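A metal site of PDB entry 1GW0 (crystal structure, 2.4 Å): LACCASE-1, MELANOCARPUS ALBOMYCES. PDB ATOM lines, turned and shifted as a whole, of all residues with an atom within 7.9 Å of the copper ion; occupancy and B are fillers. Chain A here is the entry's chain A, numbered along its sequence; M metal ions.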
ATOM      1  N   HIS A 237       8.120   1.625 -28.963  1.00  0.00           N
ATOM      2  CA  HIS A 237       9.533   1.832 -28.626  1.00  0.00           C
ATOM      3  C   HIS A 237      10.058   0.416 -28.401  1.00  0.00           C
ATOM      4  O   HIS A 237       9.463  -0.349 -27.647  1.00  0.00           O
ATOM      5  CB  HIS A 237       9.670   2.650 -27.344  1.00  0.00           C
ATOM      6  CG  HIS A 237       9.311   4.094 -27.496  1.00  0.00           C
ATOM      7  ND1 HIS A 237       8.047   4.508 -27.877  1.00  0.00           N
ATOM      8  CD2 HIS A 237      10.020   5.227 -27.270  1.00  0.00           C
ATOM      9  CE1 HIS A 237       8.003   5.828 -27.876  1.00  0.00           C
ATOM     10  NE2 HIS A 237       9.188   6.289 -27.512  1.00  0.00           N
ATOM     11  N   VAL A 361       6.258  20.606 -20.710  1.00  0.00           N
ATOM     12  CA  VAL A 361       5.326  19.785 -21.462  1.00  0.00           C
ATOM     13  C   VAL A 361       4.100  19.493 -20.591  1.00  0.00           C
ATOM     14  O   VAL A 361       4.230  19.104 -19.436  1.00  0.00           O
ATOM     15  CB  VAL A 361       5.972  18.444 -21.860  1.00  0.00           C
ATOM     16  CG1 VAL A 361       4.980  17.596 -22.644  1.00  0.00           C
ATOM     17  CG2 VAL A 361       7.214  18.707 -22.694  1.00  0.00           C
ATOM     18  N   TRP A 373      -1.835  17.974 -26.257  1.00  0.00           N
ATOM     19  CA  TRP A 373      -0.500  18.205 -25.714  1.00  0.00           C
ATOM     20  C   TRP A 373      -0.085  19.645 -25.973  1.00  0.00           C
ATOM     21  O   TRP A 373      -0.287  20.181 -27.060  1.00  0.00           O
ATOM     22  CB  TRP A 373       0.512  17.233 -26.328  1.00  0.00           C
ATOM     23  CG  TRP A 373       0.275  15.790 -25.937  1.00  0.00           C
ATOM     24  CD1 TRP A 373      -0.463  14.870 -26.626  1.00  0.00           C
ATOM     25  CD2 TRP A 373       0.729  15.122 -24.741  1.00  0.00           C
ATOM     26  NE1 TRP A 373      -0.503  13.681 -25.940  1.00  0.00           N
ATOM     27  CE2 TRP A 373       0.211  13.808 -24.784  1.00  0.00           C
ATOM     28  CE3 TRP A 373       1.508  15.516 -23.651  1.00  0.00           C
ATOM     29  CZ2 TRP A 373       0.464  12.876 -23.766  1.00  0.00           C
ATOM     30  CZ3 TRP A 373       1.753  14.590 -22.630  1.00  0.00           C
ATOM     31  CH2 TRP A 373       1.234  13.285 -22.694  1.00  0.00           C
ATOM     32  N   ASN A 421       8.706  17.335 -18.113  1.00  0.00           N
ATOM     33  CA  ASN A 421       7.584  16.479 -18.513  1.00  0.00           C
ATOM     34  C   ASN A 421       6.361  16.426 -17.601  1.00  0.00           C
ATOM     35  O   ASN A 421       6.152  15.457 -16.870  1.00  0.00           O
ATOM     36  CB  ASN A 421       8.121  15.059 -18.755  1.00  0.00           C
ATOM     37  CG  ASN A 421       7.118  14.178 -19.460  1.00  0.00           C
ATOM     38  OD1 ASN A 421       6.061  14.636 -19.909  1.00  0.00           O
ATOM     39  ND2 ASN A 421       7.442  12.890 -19.556  1.00  0.00           N
ATOM     40  N   LEU A 429       3.944  10.472 -19.331  1.00  0.00           N
ATOM     41  CA  LEU A 429       4.408   9.380 -20.186  1.00  0.00           C
ATOM     42  C   LEU A 429       5.793   9.654 -20.760  1.00  0.00           C
ATOM     43  O   LEU A 429       6.223  10.797 -20.852  1.00  0.00           O
ATOM     44  CB  LEU A 429       3.466   9.175 -21.369  1.00  0.00           C
ATOM     45  CG  LEU A 429       1.969   8.933 -21.174  1.00  0.00           C
ATOM     46  CD1 LEU A 429       1.256   9.080 -22.513  1.00  0.00           C
ATOM     47  CD2 LEU A 429       1.725   7.557 -20.581  1.00  0.00           C
ATOM     48  N   PRO A 430       6.504   8.592 -21.142  1.00  0.00           N
ATOM     49  CA  PRO A 430       7.831   8.777 -21.721  1.00  0.00           C
ATOM     50  C   PRO A 430       7.591   9.417 -23.094  1.00  0.00           C
ATOM     51  O   PRO A 430       6.625   9.068 -23.784  1.00  0.00           O
ATOM     52  CB  PRO A 430       8.360   7.350 -21.860  1.00  0.00           C
ATOM     53  CG  PRO A 430       7.668   6.613 -20.746  1.00  0.00           C
ATOM     54  CD  PRO A 430       6.268   7.171 -20.829  1.00  0.00           C
ATOM     55  N   HIS A 431       8.440  10.371 -23.480  1.00  0.00           N
ATOM     56  CA  HIS A 431       8.309  11.048 -24.778  1.00  0.00           C
ATOM     57  C   HIS A 431       9.641  11.097 -25.526  1.00  0.00           C
ATOM     58  O   HIS A 431      10.624  11.654 -25.016  1.00  0.00           O
ATOM     59  CB  HIS A 431       7.844  12.490 -24.602  1.00  0.00           C
ATOM     60  CG  HIS A 431       6.423  12.628 -24.137  1.00  0.00           C
ATOM     61  ND1 HIS A 431       5.344  12.306 -24.942  1.00  0.00           N
ATOM     62  CD2 HIS A 431       5.903  13.076 -22.971  1.00  0.00           C
ATOM     63  CE1 HIS A 431       4.234  12.555 -24.289  1.00  0.00           C
ATOM     64  NE2 HIS A 431       4.540  13.019 -23.092  1.00  0.00           N
ATOM     65  N   PRO A 432       9.714  10.496 -26.727  1.00  0.00           N
ATOM     66  CA  PRO A 432      10.967  10.533 -27.486  1.00  0.00           C
ATOM     67  C   PRO A 432      11.034  11.905 -28.160  1.00  0.00           C
ATOM     68  O   PRO A 432      10.227  12.218 -29.024  1.00  0.00           O
ATOM     69  CB  PRO A 432      10.790   9.395 -28.487  1.00  0.00           C
ATOM     70  CG  PRO A 432       9.311   9.410 -28.753  1.00  0.00           C
ATOM     71  CD  PRO A 432       8.739   9.580 -27.356  1.00  0.00           C
ATOM     72  N   MET A 433      11.989  12.730 -27.723  1.00  0.00           N
ATOM     73  CA  MET A 433      12.153  14.070 -28.280  1.00  0.00           C
ATOM     74  C   MET A 433      13.131  14.100 -29.456  1.00  0.00           C
ATOM     75  O   MET A 433      14.195  13.494 -29.398  1.00  0.00           O
ATOM     76  CB  MET A 433      12.627  15.023 -27.188  1.00  0.00           C
ATOM     77  CG  MET A 433      11.681  15.147 -25.998  1.00  0.00           C
ATOM     78  SD  MET A 433       9.992  15.577 -26.461  1.00  0.00           S
ATOM     79  CE  MET A 433      10.205  17.190 -27.211  1.00  0.00           C
ATOM     80  N   MET A 480      15.315  10.073 -25.097  1.00  0.00           N
ATOM     81  CA  MET A 480      14.114   9.947 -24.261  1.00  0.00           C
ATOM     82  C   MET A 480      13.937  10.977 -23.135  1.00  0.00           C
ATOM     83  O   MET A 480      14.884  11.324 -22.425  1.00  0.00           O
ATOM     84  CB  MET A 480      14.039   8.543 -23.648  1.00  0.00           C
ATOM     85  CG  MET A 480      13.708   7.424 -24.644  1.00  0.00           C
ATOM     86  SD  MET A 480      12.211   7.758 -25.567  1.00  0.00           S
ATOM     87  CE  MET A 480      10.928   7.643 -24.326  1.00  0.00           C
ATOM     88  N   LEU A 481      12.708  11.443 -22.987  1.00  0.00           N
ATOM     89  CA  LEU A 481      12.362  12.367 -21.921  1.00  0.00           C
ATOM     90  C   LEU A 481      11.745  11.484 -20.832  1.00  0.00           C
ATOM     91  O   LEU A 481      10.680  10.914 -21.029  1.00  0.00           O
ATOM     92  CB  LEU A 481      11.322  13.379 -22.413  1.00  0.00           C
ATOM     93  CG  LEU A 481      10.741  14.295 -21.326  1.00  0.00           C
ATOM     94  CD1 LEU A 481      11.833  15.232 -20.819  1.00  0.00           C
ATOM     95  CD2 LEU A 481       9.579  15.085 -21.900  1.00  0.00           C
ATOM     96  N   HIS A 502      10.085  18.283 -31.729  1.00  0.00           N
ATOM     97  CA  HIS A 502       8.851  17.648 -31.310  1.00  0.00           C
ATOM     98  C   HIS A 502       9.026  16.245 -30.775  1.00  0.00           C
ATOM     99  O   HIS A 502      10.129  15.704 -30.783  1.00  0.00           O
ATOM    100  CB  HIS A 502       7.883  17.631 -32.497  1.00  0.00           C
ATOM    101  CG  HIS A 502       8.396  16.903 -33.702  1.00  0.00           C
ATOM    102  ND1 HIS A 502       8.339  15.530 -33.832  1.00  0.00           N
ATOM    103  CD2 HIS A 502       8.988  17.351 -34.839  1.00  0.00           C
ATOM    104  CE1 HIS A 502       8.855  15.173 -34.985  1.00  0.00           C
ATOM    105  NE2 HIS A 502       9.263  16.254 -35.625  1.00  0.00           N
ATOM    106  N   CYS A 503       7.937  15.673 -30.273  1.00  0.00           N
ATOM    107  CA  CYS A 503       7.944  14.298 -29.787  1.00  0.00           C
ATOM    108  C   CYS A 503       7.661  13.485 -31.046  1.00  0.00           C
ATOM    109  O   CYS A 503       6.765  13.843 -31.815  1.00  0.00           O
ATOM    110  CB  CYS A 503       6.843  14.062 -28.763  1.00  0.00           C
ATOM    111  SG  CYS A 503       6.577  12.318 -28.423  1.00  0.00           S
ATOM    112  N   HIS A 504       8.391  12.391 -31.269  1.00  0.00           N
ATOM    113  CA  HIS A 504       8.174  11.610 -32.489  1.00  0.00           C
ATOM    114  C   HIS A 504       7.044  10.594 -32.460  1.00  0.00           C
ATOM    115  O   HIS A 504       6.877   9.833 -33.403  1.00  0.00           O
ATOM    116  CB  HIS A 504       9.473  10.927 -32.928  1.00  0.00           C
ATOM    117  CG  HIS A 504       9.690  10.967 -34.412  1.00  0.00           C
ATOM    118  ND1 HIS A 504       8.876  10.299 -35.304  1.00  0.00           N
ATOM    119  CD2 HIS A 504      10.625  11.609 -35.159  1.00  0.00           C
ATOM    120  CE1 HIS A 504       9.305  10.528 -36.535  1.00  0.00           C
ATOM    121  NE2 HIS A 504      10.355  11.316 -36.480  1.00  0.00           N
ATOM    122  N   ILE A 505       6.281  10.558 -31.368  1.00  0.00           N
ATOM    123  CA  ILE A 505       5.148   9.651 -31.323  1.00  0.00           C
ATOM    124  C   ILE A 505       4.089  10.386 -32.151  1.00  0.00           C
ATOM    125  O   ILE A 505       3.666  11.486 -31.785  1.00  0.00           O
ATOM    126  CB  ILE A 505       4.627   9.429 -29.891  1.00  0.00           C
ATOM    127  CG1 ILE A 505       5.593   8.504 -29.133  1.00  0.00           C
ATOM    128  CG2 ILE A 505       3.225   8.820 -29.920  1.00  0.00           C
ATOM    129  CD1 ILE A 505       5.243   8.287 -27.677  1.00  0.00           C
ATOM    130  N   ALA A 506       3.699   9.794 -33.272  1.00  0.00           N
ATOM    131  CA  ALA A 506       2.730  10.422 -34.167  1.00  0.00           C
ATOM    132  C   ALA A 506       1.516  11.019 -33.453  1.00  0.00           C
ATOM    133  O   ALA A 506       1.155  12.178 -33.660  1.00  0.00           O
ATOM    134  CB  ALA A 506       2.271   9.424 -35.225  1.00  0.00           C
ATOM    135  N   TRP A 507       0.902  10.211 -32.589  1.00  0.00           N
ATOM    136  CA  TRP A 507      -0.276  10.630 -31.873  1.00  0.00           C
ATOM    137  C   TRP A 507      -0.058  11.931 -31.072  1.00  0.00           C
ATOM    138  O   TRP A 507      -0.945  12.774 -31.000  1.00  0.00           O
ATOM    139  CB  TRP A 507      -0.721   9.494 -30.929  1.00  0.00           C
ATOM    140  CG  TRP A 507      -0.595   8.094 -31.514  1.00  0.00           C
ATOM    141  CD1 TRP A 507      -0.226   6.968 -30.848  1.00  0.00           C
ATOM    142  CD2 TRP A 507      -0.833   7.695 -32.881  1.00  0.00           C
ATOM    143  NE1 TRP A 507      -0.211   5.888 -31.698  1.00  0.00           N
ATOM    144  CE2 TRP A 507      -0.585   6.297 -32.951  1.00  0.00           C
ATOM    145  CE3 TRP A 507      -1.230   8.357 -34.048  1.00  0.00           C
ATOM    146  CZ2 TRP A 507      -0.718   5.561 -34.142  1.00  0.00           C
ATOM    147  CZ3 TRP A 507      -1.365   7.631 -35.229  1.00  0.00           C
ATOM    148  CH2 TRP A 507      -1.098   6.239 -35.260  1.00  0.00           C
ATOM    149  N   HIS A 508       1.136  12.084 -30.496  1.00  0.00           N
ATOM    150  CA  HIS A 508       1.457  13.256 -29.681  1.00  0.00           C
ATOM    151  C   HIS A 508       1.760  14.542 -30.464  1.00  0.00           C
ATOM    152  O   HIS A 508       1.183  15.596 -30.168  1.00  0.00           O
ATOM    153  CB  HIS A 508       2.647  12.940 -28.767  1.00  0.00           C
ATOM    154  CG  HIS A 508       2.374  11.826 -27.797  1.00  0.00           C
ATOM    155  ND1 HIS A 508       3.369  11.224 -27.066  1.00  0.00           N
ATOM    156  CD2 HIS A 508       1.221  11.197 -27.457  1.00  0.00           C
ATOM    157  CE1 HIS A 508       2.854  10.274 -26.314  1.00  0.00           C
ATOM    158  NE2 HIS A 508       1.550  10.238 -26.536  1.00  0.00           N
ATOM    159  N   VAL A 509       2.671  14.473 -31.432  1.00  0.00           N
ATOM    160  CA  VAL A 509       3.006  15.654 -32.230  1.00  0.00           C
ATOM    161  C   VAL A 509       1.720  16.115 -32.916  1.00  0.00           C
ATOM    162  O   VAL A 509       1.450  17.306 -33.046  1.00  0.00           O
ATOM    163  CB  VAL A 509       4.073  15.329 -33.311  1.00  0.00           C
ATOM    164  CG1 VAL A 509       3.475  14.443 -34.413  1.00  0.00           C
ATOM    165  CG2 VAL A 509       4.649  16.614 -33.883  1.00  0.00           C
ATOM    166  N   LEU A 513       2.389  18.341 -29.358  1.00  0.00           N
ATOM    167  CA  LEU A 513       3.665  18.333 -28.649  1.00  0.00           C
ATOM    168  C   LEU A 513       4.818  18.739 -29.566  1.00  0.00           C
ATOM    169  O   LEU A 513       5.476  17.885 -30.170  1.00  0.00           O
ATOM    170  CB  LEU A 513       3.927  16.947 -28.052  1.00  0.00           C
ATOM    171  CG  LEU A 513       4.654  16.985 -26.706  1.00  0.00           C
ATOM    172  CD1 LEU A 513       4.569  15.618 -26.019  1.00  0.00           C
ATOM    173  CD2 LEU A 513       6.100  17.407 -26.921  1.00  0.00           C
HETATM  174 CU    CU M   1       5.092  12.061 -26.820  1.00  0.00          CU
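The backbone NH (N) of Leu 481 is in hydrogen-bond range of the backbone carbonyl oxygen (O) of His 431 (2.9 Å).
The backbone carbonyl oxygen of Leu 513 is in hydrogen-bond range of the backbone NH of Cys 503 (3.3 Å).
N of Leu 513 is in hydrogen-bond range of O of His 508, at 3.1 Å.
The side-chain sulfur (SG) of Cys 503 lies close to the backbone carbonyl oxygen (O) of Pro 432, at 3.7 Å.
N of Ile 505 lies close to SG of Cys 503 (3.4 Å).
Ile 505 touches the copper ion.
Leu 513 touches the copper ion (CD1 to CU, 3.7 Å).
Of the 20 residues printed, 5 come within 4 Å of the copper ion.
The nearest printed residue that does not touch the copper ion is Pro 432 (4.4 Å).
The copper ion is bound by ND1 of His 431 (1.9 Å), ND1 of His 508 (1.9 Å) and SG of Cys 503 (2.2 Å).
The copper ion has three donor atoms within binding distance.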
